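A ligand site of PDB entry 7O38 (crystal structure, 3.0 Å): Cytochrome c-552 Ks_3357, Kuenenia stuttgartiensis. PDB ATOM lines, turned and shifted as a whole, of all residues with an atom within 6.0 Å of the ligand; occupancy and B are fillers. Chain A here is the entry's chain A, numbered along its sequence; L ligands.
SG of Cys 15 is bonded to C18 of the ligand. The side-chain sulfur of Cys 18 is bonded to a carbon (C25) of the ligand (1.8 Å). FE1 of the ligand is bound by NE2 of His 19, 2.3 Å away. An oxygen (O2) of the ligand lies within hydrogen-bond range of the side-chain hydroxyl (OG) of Ser 54 (2.6 Å). O4 of the ligand lies within hydrogen-bond range of ND2 of Asn 60 (2.8 Å). An oxygen (O2) of the ligand lies within salt-bridge range of the side-chain amino group (NZ) of Lys 59 (3.2 Å). An oxygen (O1) of the ligand is in salt-bridge range of the side-chain amino group of Lys 46.
The side-chain hydroxyl (OG) of Ser 54 lies within hydrogen-bond range of the backbone carbonyl oxygen (O) of Glu 50 (3.3 Å). The backbone NH of Trp 65 lies within hydrogen-bond range of the backbone carbonyl oxygen of Ile 55, 2.9 Å away. O of Gly 29 sits at hydrogen-bond distance from N of Ala 34.
Residues that only touch the ligand: His 14 (3.5 Å), Leu 32 (3.0 Å), Lys 33 (3.7 Å), Ala 34 (3.5 Å), Pro 35 (3.6 Å), Leu 37 (3.9 Å), Trp 42 (3.3 Å), Ile 51 (3.6 Å), Ile 55 (3.7 Å), Met 62 (3.9 Å), Trp 65 (3.5 Å) and Leu 69 (3.98 Å). 19 residues have an atom within 4 Å of the ligand: His 14, Cys 15, Cys 18, His 19, Leu 32, Lys 33, Ala 34, Pro 35, Leu 37, Trp 42, Lys 46, Ile 51, Ser 54, Ile 55, Lys 59, Asn 60, Met 62, Trp 65 and Leu 69.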
ATOM      1  N   LEU A  10      25.779   9.135   6.225  1.00  0.00           N
ATOM      2  CA  LEU A  10      24.696   9.891   6.850  1.00  0.00           C
ATOM      3  C   LEU A  10      24.551   9.501   8.306  1.00  0.00           C
ATOM      4  O   LEU A  10      24.456  10.356   9.189  1.00  0.00           O
ATOM      5  CB  LEU A  10      23.375   9.660   6.110  1.00  0.00           C
ATOM      6  CG  LEU A  10      23.197  10.327   4.769  1.00  0.00           C
ATOM      7  CD1 LEU A  10      21.871   9.866   4.214  1.00  0.00           C
ATOM      8  CD2 LEU A  10      23.240  11.824   4.902  1.00  0.00           C
ATOM      9  N   PHE A  11      24.585   8.198   8.592  1.00  0.00           N
ATOM     10  CA  PHE A  11      24.374   7.731   9.957  1.00  0.00           C
ATOM     11  C   PHE A  11      25.435   8.284  10.895  1.00  0.00           C
ATOM     12  O   PHE A  11      25.126   8.781  11.975  1.00  0.00           O
ATOM     13  CB  PHE A  11      24.361   6.201   9.998  1.00  0.00           C
ATOM     14  CG  PHE A  11      24.068   5.637  11.373  1.00  0.00           C
ATOM     15  CD1 PHE A  11      25.117   5.399  12.270  1.00  0.00           C
ATOM     16  CD2 PHE A  11      22.773   5.306  11.749  1.00  0.00           C
ATOM     17  CE1 PHE A  11      24.855   4.874  13.525  1.00  0.00           C
ATOM     18  CE2 PHE A  11      22.514   4.755  13.017  1.00  0.00           C
ATOM     19  CZ  PHE A  11      23.559   4.546  13.891  1.00  0.00           C
ATOM     20  N   HIS A  14      24.895  12.086  11.480  1.00  0.00           N
ATOM     21  CA  HIS A  14      23.628  12.457  12.112  1.00  0.00           C
ATOM     22  C   HIS A  14      23.349  11.669  13.390  1.00  0.00           C
ATOM     23  O   HIS A  14      22.850  12.227  14.367  1.00  0.00           O
ATOM     24  CB  HIS A  14      22.467  12.271  11.131  1.00  0.00           C
ATOM     25  CG  HIS A  14      22.473  13.212   9.973  1.00  0.00           C
ATOM     26  ND1 HIS A  14      22.386  14.576  10.125  1.00  0.00           N
ATOM     27  CD2 HIS A  14      22.487  12.984   8.638  1.00  0.00           C
ATOM     28  CE1 HIS A  14      22.376  15.149   8.943  1.00  0.00           C
ATOM     29  NE2 HIS A  14      22.448  14.212   8.013  1.00  0.00           N
ATOM     30  N   CYS A  15      23.617  10.365  13.370  1.00  0.00           N
ATOM     31  CA  CYS A  15      22.976   9.416  14.279  1.00  0.00           C
ATOM     32  C   CYS A  15      23.936   8.842  15.296  1.00  0.00           C
ATOM     33  O   CYS A  15      23.587   8.718  16.463  1.00  0.00           O
ATOM     34  CB  CYS A  15      22.426   8.243  13.490  1.00  0.00           C
ATOM     35  SG  CYS A  15      21.298   8.725  12.227  1.00  0.00           S
ATOM     36  N   ALA A  16      25.146   8.487  14.853  1.00  0.00           N
ATOM     37  CA  ALA A  16      26.144   7.896  15.736  1.00  0.00           C
ATOM     38  C   ALA A  16      26.402   8.736  16.989  1.00  0.00           C
ATOM     39  O   ALA A  16      26.913   8.197  17.978  1.00  0.00           O
ATOM     40  CB  ALA A  16      27.449   7.696  14.972  1.00  0.00           C
ATOM     41  N   LYS A  17      26.058  10.037  16.977  1.00  0.00           N
ATOM     42  CA  LYS A  17      26.126  10.886  18.167  1.00  0.00           C
ATOM     43  C   LYS A  17      25.578  10.134  19.379  1.00  0.00           C
ATOM     44  O   LYS A  17      26.178  10.195  20.467  1.00  0.00           O
ATOM     45  CB  LYS A  17      25.322  12.188  17.965  1.00  0.00           C
ATOM     46  CG  LYS A  17      25.943  13.178  16.996  1.00  0.00           C
ATOM     47  CD  LYS A  17      25.009  14.316  16.598  1.00  0.00           C
ATOM     48  CE  LYS A  17      25.733  15.226  15.553  1.00  0.00           C
ATOM     49  NZ  LYS A  17      24.899  16.239  14.830  1.00  0.00           N
ATOM     50  N   CYS A  18      24.500   9.383  19.196  1.00  0.00           N
ATOM     51  CA  CYS A  18      23.795   8.702  20.283  1.00  0.00           C
ATOM     52  C   CYS A  18      23.904   7.193  20.197  1.00  0.00           C
ATOM     53  O   CYS A  18      24.203   6.539  21.201  1.00  0.00           O
ATOM     54  CB  CYS A  18      22.315   9.094  20.256  1.00  0.00           C
ATOM     55  SG  CYS A  18      22.035  10.838  20.549  1.00  0.00           S
ATOM     56  N   HIS A  19      23.651   6.603  19.034  1.00  0.00           N
ATOM     57  CA  HIS A  19      23.627   5.153  18.899  1.00  0.00           C
ATOM     58  C   HIS A  19      25.008   4.544  18.764  1.00  0.00           C
ATOM     59  O   HIS A  19      25.126   3.315  18.774  1.00  0.00           O
ATOM     60  CB  HIS A  19      22.773   4.792  17.705  1.00  0.00           C
ATOM     61  CG  HIS A  19      21.374   5.275  17.844  1.00  0.00           C
ATOM     62  ND1 HIS A  19      20.448   4.647  18.633  1.00  0.00           N
ATOM     63  CD2 HIS A  19      20.764   6.369  17.345  1.00  0.00           C
ATOM     64  CE1 HIS A  19      19.313   5.304  18.597  1.00  0.00           C
ATOM     65  NE2 HIS A  19      19.481   6.351  17.814  1.00  0.00           N
ATOM     66  N   GLY A  29      24.111   8.473  24.274  1.00  0.00           N
ATOM     67  CA  GLY A  29      22.863   7.759  24.011  1.00  0.00           C
ATOM     68  C   GLY A  29      22.290   7.071  25.242  1.00  0.00           C
ATOM     69  O   GLY A  29      21.106   7.183  25.530  1.00  0.00           O
ATOM     70  N   LEU A  32      20.308   9.328  27.389  1.00  0.00           N
ATOM     71  CA  LEU A  32      19.002   9.649  26.842  1.00  0.00           C
ATOM     72  C   LEU A  32      18.113   8.403  26.688  1.00  0.00           C
ATOM     73  O   LEU A  32      17.084   8.464  25.995  1.00  0.00           O
ATOM     74  CB  LEU A  32      19.177  10.343  25.485  1.00  0.00           C
ATOM     75  CG  LEU A  32      20.072  11.574  25.509  1.00  0.00           C
ATOM     76  CD1 LEU A  32      20.488  11.883  24.117  1.00  0.00           C
ATOM     77  CD2 LEU A  32      19.325  12.743  26.067  1.00  0.00           C
ATOM     78  N   LYS A  33      18.478   7.299  27.336  1.00  0.00           N
ATOM     79  CA  LYS A  33      17.681   6.083  27.280  1.00  0.00           C
ATOM     80  C   LYS A  33      17.559   5.567  25.845  1.00  0.00           C
ATOM     81  O   LYS A  33      16.488   5.135  25.415  1.00  0.00           O
ATOM     82  CB  LYS A  33      16.296   6.290  27.891  1.00  0.00           C
ATOM     83  CG  LYS A  33      16.255   6.959  29.262  1.00  0.00           C
ATOM     84  CD  LYS A  33      16.844   6.121  30.356  1.00  0.00           C
ATOM     85  CE  LYS A  33      16.507   6.767  31.693  1.00  0.00           C
ATOM     86  NZ  LYS A  33      17.028   5.974  32.838  1.00  0.00           N
ATOM     87  N   ALA A  34      18.652   5.657  25.078  1.00  0.00           N
ATOM     88  CA  ALA A  34      18.635   5.099  23.732  1.00  0.00           C
ATOM     89  C   ALA A  34      18.723   3.567  23.779  1.00  0.00           C
ATOM     90  O   ALA A  34      19.374   3.003  24.658  1.00  0.00           O
ATOM     91  CB  ALA A  34      19.792   5.637  22.907  1.00  0.00           C
ATOM     92  N   PRO A  35      18.118   2.895  22.815  1.00  0.00           N
ATOM     93  CA  PRO A  35      18.320   1.451  22.679  1.00  0.00           C
ATOM     94  C   PRO A  35      19.651   1.159  21.993  1.00  0.00           C
ATOM     95  O   PRO A  35      20.285   2.035  21.401  1.00  0.00           O
ATOM     96  CB  PRO A  35      17.154   1.037  21.800  1.00  0.00           C
ATOM     97  CG  PRO A  35      16.989   2.181  20.903  1.00  0.00           C
ATOM     98  CD  PRO A  35      17.344   3.423  21.687  1.00  0.00           C
ATOM     99  N   LEU A  37      20.776  -0.272  18.905  1.00  0.00           N
ATOM    100  CA  LEU A  37      20.359  -0.737  17.589  1.00  0.00           C
ATOM    101  C   LEU A  37      21.026  -2.060  17.235  1.00  0.00           C
ATOM    102  O   LEU A  37      20.451  -2.872  16.494  1.00  0.00           O
ATOM    103  CB  LEU A  37      20.651   0.323  16.520  1.00  0.00           C
ATOM    104  CG  LEU A  37      20.032   1.734  16.608  1.00  0.00           C
ATOM    105  CD1 LEU A  37      20.405   2.568  15.400  1.00  0.00           C
ATOM    106  CD2 LEU A  37      18.520   1.712  16.747  1.00  0.00           C
ATOM    107  N   TRP A  42      16.708  -6.229  20.329  1.00  0.00           N
ATOM    108  CA  TRP A  42      16.003  -5.012  19.957  1.00  0.00           C
ATOM    109  C   TRP A  42      15.572  -5.055  18.494  1.00  0.00           C
ATOM    110  O   TRP A  42      14.418  -4.741  18.161  1.00  0.00           O
ATOM    111  CB  TRP A  42      16.881  -3.780  20.223  1.00  0.00           C
ATOM    112  CG  TRP A  42      16.177  -2.528  19.838  1.00  0.00           C
ATOM    113  CD1 TRP A  42      15.374  -1.764  20.630  1.00  0.00           C
ATOM    114  CD2 TRP A  42      16.190  -1.915  18.549  1.00  0.00           C
ATOM    115  NE1 TRP A  42      14.897  -0.695  19.908  1.00  0.00           N
ATOM    116  CE2 TRP A  42      15.379  -0.769  18.622  1.00  0.00           C
ATOM    117  CE3 TRP A  42      16.813  -2.223  17.332  1.00  0.00           C
ATOM    118  CZ2 TRP A  42      15.167   0.059  17.543  1.00  0.00           C
ATOM    119  CZ3 TRP A  42      16.610  -1.399  16.250  1.00  0.00           C
ATOM    120  CH2 TRP A  42      15.787  -0.276  16.361  1.00  0.00           C
ATOM    121  N   LYS A  46      11.115  -4.593  16.616  1.00  0.00           N
ATOM    122  CA  LYS A  46      10.619  -3.508  15.786  1.00  0.00           C
ATOM    123  C   LYS A  46      10.454  -3.993  14.354  1.00  0.00           C
ATOM    124  O   LYS A  46      11.181  -4.881  13.908  1.00  0.00           O
ATOM    125  CB  LYS A  46      11.573  -2.315  15.802  1.00  0.00           C
ATOM    126  CG  LYS A  46      11.903  -1.795  17.166  1.00  0.00           C
ATOM    127  CD  LYS A  46      10.710  -1.094  17.762  1.00  0.00           C
ATOM    128  CE  LYS A  46      10.927  -0.852  19.231  1.00  0.00           C
ATOM    129  NZ  LYS A  46       9.736  -0.138  19.810  1.00  0.00           N
ATOM    130  N   GLU A  50       7.852   0.544  11.445  1.00  0.00           N
ATOM    131  CA  GLU A  50       8.065   1.212  12.716  1.00  0.00           C
ATOM    132  C   GLU A  50       9.341   2.049  12.702  1.00  0.00           C
ATOM    133  O   GLU A  50       9.353   3.190  13.181  1.00  0.00           O
ATOM    134  CB  GLU A  50       8.088   0.174  13.846  1.00  0.00           C
ATOM    135  CG  GLU A  50       6.714  -0.357  14.238  1.00  0.00           C
ATOM    136  CD  GLU A  50       6.761  -1.314  15.415  1.00  0.00           C
ATOM    137  OE1 GLU A  50       7.865  -1.810  15.764  1.00  0.00           O
ATOM    138  OE2 GLU A  50       5.687  -1.574  16.014  1.00  0.00           O
ATOM    139  N   ILE A  51      10.435   1.508  12.159  1.00  0.00           N
ATOM    140  CA  ILE A  51      11.673   2.264  12.132  1.00  0.00           C
ATOM    141  C   ILE A  51      11.532   3.483  11.250  1.00  0.00           C
ATOM    142  O   ILE A  51      11.862   4.600  11.654  1.00  0.00           O
ATOM    143  CB  ILE A  51      12.812   1.368  11.653  1.00  0.00           C
ATOM    144  CG1 ILE A  51      13.148   0.360  12.734  1.00  0.00           C
ATOM    145  CG2 ILE A  51      13.993   2.225  11.317  1.00  0.00           C
ATOM    146  CD1 ILE A  51      14.040  -0.737  12.275  1.00  0.00           C
ATOM    147  N   SER A  54       9.615   6.162  13.031  1.00  0.00           N
ATOM    148  CA  SER A  54      10.249   6.817  14.141  1.00  0.00           C
ATOM    149  C   SER A  54      11.359   7.741  13.675  1.00  0.00           C
ATOM    150  O   SER A  54      11.630   8.769  14.306  1.00  0.00           O
ATOM    151  CB  SER A  54      10.741   5.766  15.115  1.00  0.00           C
ATOM    152  OG  SER A  54       9.648   5.219  15.814  1.00  0.00           O
ATOM    153  N   ILE A  55      12.044   7.406  12.577  1.00  0.00           N
ATOM    154  CA  ILE A  55      13.009   8.361  12.058  1.00  0.00           C
ATOM    155  C   ILE A  55      12.283   9.560  11.456  1.00  0.00           C
ATOM    156  O   ILE A  55      12.677  10.716  11.652  1.00  0.00           O
ATOM    157  CB  ILE A  55      13.971   7.704  11.049  1.00  0.00           C
ATOM    158  CG1 ILE A  55      14.699   6.523  11.676  1.00  0.00           C
ATOM    159  CG2 ILE A  55      14.978   8.712  10.567  1.00  0.00           C
ATOM    160  CD1 ILE A  55      15.295   5.578  10.674  1.00  0.00           C
ATOM    161  N   LYS A  59      10.728   9.759  18.138  1.00  0.00           N
ATOM    162  CA  LYS A  59       9.974   8.762  18.855  1.00  0.00           C
ATOM    163  C   LYS A  59       9.228   8.953  20.177  1.00  0.00           C
ATOM    164  O   LYS A  59       7.991   8.935  20.120  1.00  0.00           O
ATOM    165  CB  LYS A  59      10.971   7.617  19.118  1.00  0.00           C
ATOM    166  CG  LYS A  59      10.476   6.458  19.944  1.00  0.00           C
ATOM    167  CD  LYS A  59       9.456   5.597  19.331  1.00  0.00           C
ATOM    168  CE  LYS A  59       9.185   4.449  20.272  1.00  0.00           C
ATOM    169  NZ  LYS A  59       8.132   3.566  19.741  1.00  0.00           N
ATOM    170  N   ASN A  60       9.823   9.250  21.333  1.00  0.00           N
ATOM    171  CA  ASN A  60       8.962   9.775  22.388  1.00  0.00           C
ATOM    172  C   ASN A  60       9.144  11.249  22.671  1.00  0.00           C
ATOM    173  O   ASN A  60       8.275  12.089  22.410  1.00  0.00           O
ATOM    174  CB  ASN A  60       9.141   8.920  23.653  1.00  0.00           C
ATOM    175  CG  ASN A  60       8.591   7.487  23.477  1.00  0.00           C
ATOM    176  OD1 ASN A  60       7.683   7.242  22.672  1.00  0.00           O
ATOM    177  ND2 ASN A  60       9.172   6.538  24.191  1.00  0.00           N
ATOM    178  N   LYS A  61      10.369  11.580  23.085  1.00  0.00           N
ATOM    179  CA  LYS A  61      10.864  12.923  23.280  1.00  0.00           C
ATOM    180  C   LYS A  61      11.830  13.250  22.184  1.00  0.00           C
ATOM    181  O   LYS A  61      12.435  14.326  22.204  1.00  0.00           O
ATOM    182  CB  LYS A  61      11.536  13.038  24.650  1.00  0.00           C
ATOM    183  CG  LYS A  61      10.581  12.812  25.842  1.00  0.00           C
ATOM    184  CD  LYS A  61      11.295  12.934  27.187  1.00  0.00           C
ATOM    185  CE  LYS A  61      10.330  12.750  28.358  1.00  0.00           C
ATOM    186  NZ  LYS A  61       9.793  11.359  28.429  1.00  0.00           N
ATOM    187  N   MET A  62      11.979  12.394  21.292  1.00  0.00           N
ATOM    188  CA  MET A  62      13.065  12.612  20.370  1.00  0.00           C
ATOM    189  C   MET A  62      12.520  13.217  19.089  1.00  0.00           C
ATOM    190  O   MET A  62      11.340  13.032  18.745  1.00  0.00           O
ATOM    191  CB  MET A  62      13.812  11.309  20.081  1.00  0.00           C
ATOM    192  CG  MET A  62      14.568  10.819  21.294  1.00  0.00           C
ATOM    193  SD  MET A  62      15.954  11.917  21.680  1.00  0.00           S
ATOM    194  CE  MET A  62      15.665  12.284  23.412  1.00  0.00           C
ATOM    195  N   TRP A  65      13.324  13.550  11.982  1.00  0.00           N
ATOM    196  CA  TRP A  65      14.363  13.865  11.018  1.00  0.00           C
ATOM    197  C   TRP A  65      13.824  14.225   9.647  1.00  0.00           C
ATOM    198  O   TRP A  65      14.635  14.449   8.726  1.00  0.00           O
ATOM    199  CB  TRP A  65      15.319  12.693  10.895  1.00  0.00           C
ATOM    200  CG  TRP A  65      16.226  12.566  12.058  1.00  0.00           C
ATOM    201  CD1 TRP A  65      16.026  11.781  13.158  1.00  0.00           C
ATOM    202  CD2 TRP A  65      17.492  13.205  12.249  1.00  0.00           C
ATOM    203  NE1 TRP A  65      17.093  11.899  14.013  1.00  0.00           N
ATOM    204  CE2 TRP A  65      18.007  12.768  13.480  1.00  0.00           C
ATOM    205  CE3 TRP A  65      18.242  14.111  11.490  1.00  0.00           C
ATOM    206  CZ2 TRP A  65      19.228  13.219  13.986  1.00  0.00           C
ATOM    207  CZ3 TRP A  65      19.458  14.553  11.994  1.00  0.00           C
ATOM    208  CH2 TRP A  65      19.939  14.110  13.229  1.00  0.00           C
ATOM    209  N   LEU A  69      16.402  15.400   6.484  1.00  0.00           N
ATOM    210  CA  LEU A  69      16.697  14.286   5.592  1.00  0.00           C
ATOM    211  C   LEU A  69      15.549  14.083   4.604  1.00  0.00           C
ATOM    212  O   LEU A  69      14.379  14.267   4.960  1.00  0.00           O
ATOM    213  CB  LEU A  69      16.928  12.998   6.372  1.00  0.00           C
ATOM    214  CG  LEU A  69      17.946  13.012   7.510  1.00  0.00           C
ATOM    215  CD1 LEU A  69      17.912  11.690   8.228  1.00  0.00           C
ATOM    216  CD2 LEU A  69      19.343  13.315   7.019  1.00  0.00           C
ATOM    217  N   LEU A  77      18.691   5.036   5.503  1.00  0.00           N
ATOM    218  CA  LEU A  77      19.042   4.925   6.910  1.00  0.00           C
ATOM    219  C   LEU A  77      18.316   3.775   7.596  1.00  0.00           C
ATOM    220  O   LEU A  77      18.924   3.017   8.363  1.00  0.00           O
ATOM    221  CB  LEU A  77      18.748   6.241   7.601  1.00  0.00           C
ATOM    222  CG  LEU A  77      19.859   7.202   7.299  1.00  0.00           C
ATOM    223  CD1 LEU A  77      19.351   8.585   7.519  1.00  0.00           C
ATOM    224  CD2 LEU A  77      21.009   6.904   8.208  1.00  0.00           C
ATOM    225  N   ALA A  78      17.011   3.633   7.343  1.00  0.00           N
ATOM    226  CA  ALA A  78      16.287   2.520   7.935  1.00  0.00           C
ATOM    227  C   ALA A  78      16.956   1.206   7.530  1.00  0.00           C
ATOM    228  O   ALA A  78      17.264   0.371   8.386  1.00  0.00           O
ATOM    229  CB  ALA A  78      14.823   2.547   7.517  1.00  0.00           C
ATOM    230  N   VAL A  81      20.153   0.888   9.519  1.00  0.00           N
ATOM    231  CA  VAL A  81      19.941   0.506  10.914  1.00  0.00           C
ATOM    232  C   VAL A  81      19.827  -1.010  11.016  1.00  0.00           C
ATOM    233  O   VAL A  81      20.341  -1.620  11.957  1.00  0.00           O
ATOM    234  CB  VAL A  81      18.693   1.205  11.467  1.00  0.00           C
ATOM    235  CG1 VAL A  81      18.322   0.640  12.801  1.00  0.00           C
ATOM    236  CG2 VAL A  81      18.951   2.691  11.544  1.00  0.00           C
HETATM  237 FE1  LIG L   1      17.488   7.483  17.470  1.00  0.00          FE
HETATM  238  C1  LIG L   1      15.248   5.600  19.000  1.00  0.00           C
HETATM  239  C2  LIG L   1      17.387   5.650  14.658  1.00  0.00           C
HETATM  240  C3  LIG L   1      19.313   9.875  15.782  1.00  0.00           C
HETATM  241  C4  LIG L   1      18.444   8.904  20.430  1.00  0.00           C
HETATM  242  N1  LIG L   1      16.519   5.939  16.925  1.00  0.00           N
HETATM  243  C5  LIG L   1      15.582   5.262  17.705  1.00  0.00           C
HETATM  244  C6  LIG L   1      15.062   4.165  16.908  1.00  0.00           C
HETATM  245  C7  LIG L   1      15.653   4.192  15.714  1.00  0.00           C
HETATM  246  C8  LIG L   1      16.578   5.303  15.705  1.00  0.00           C
HETATM  247  C9  LIG L   1      15.426   3.241  14.502  1.00  0.00           C
HETATM  248  C10 LIG L   1      13.986   3.174  17.353  1.00  0.00           C
HETATM  249  C11 LIG L   1      12.629   3.797  17.072  1.00  0.00           C
HETATM  250  C12 LIG L   1      11.536   2.994  17.710  1.00  0.00           C
HETATM  251  O1  LIG L   1      11.831   2.066  18.493  1.00  0.00           O
HETATM  252  O2  LIG L   1      10.344   3.294  17.431  1.00  0.00           O
HETATM  253  N2  LIG L   1      18.232   7.699  15.591  1.00  0.00           N
HETATM  254  C13 LIG L   1      18.033   6.838  14.564  1.00  0.00           C
HETATM  255  C14 LIG L   1      18.571   7.384  13.346  1.00  0.00           C
HETATM  256  C15 LIG L   1      19.129   8.546  13.653  1.00  0.00           C
HETATM  257  C16 LIG L   1      18.912   8.777  15.061  1.00  0.00           C
HETATM  258  C17 LIG L   1      18.531   6.687  11.969  1.00  0.00           C
HETATM  259  C18 LIG L   1      19.808   9.542  12.687  1.00  0.00           C
HETATM  260  C19 LIG L   1      19.125   9.985  11.618  1.00  0.00           C
HETATM  261  N3  LIG L   1      18.639   9.081  17.980  1.00  0.00           N
HETATM  262  C20 LIG L   1      19.336   9.936  17.144  1.00  0.00           C
HETATM  263  C21 LIG L   1      20.084  10.879  17.953  1.00  0.00           C
HETATM  264  C22 LIG L   1      19.841  10.576  19.227  1.00  0.00           C
HETATM  265  C23 LIG L   1      18.917   9.469  19.278  1.00  0.00           C
HETATM  266  C24 LIG L   1      21.011  11.982  17.391  1.00  0.00           C
HETATM  267  C25 LIG L   1      20.324  11.274  20.505  1.00  0.00           C
HETATM  268  C26 LIG L   1      20.522  12.595  20.531  1.00  0.00           C
HETATM  269  N4  LIG L   1      16.976   7.278  19.369  1.00  0.00           N
HETATM  270  C27 LIG L   1      17.444   7.969  20.461  1.00  0.00           C
HETATM  271  C28 LIG L   1      16.709   7.567  21.629  1.00  0.00           C
HETATM  272  C29 LIG L   1      15.815   6.652  21.254  1.00  0.00           C
HETATM  273  C30 LIG L   1      15.971   6.455  19.812  1.00  0.00           C
HETATM  274  C31 LIG L   1      16.939   8.116  23.035  1.00  0.00           C
HETATM  275  C32 LIG L   1      14.803   5.952  22.175  1.00  0.00           C
HETATM  276  C33 LIG L   1      13.599   6.869  22.315  1.00  0.00           C
HETATM  277  C34 LIG L   1      12.496   6.210  23.114  1.00  0.00           C
HETATM  278  O3  LIG L   1      12.136   5.022  22.884  1.00  0.00           O
HETATM  279  O4  LIG L   1      11.921   6.888  23.986  1.00  0.00           O
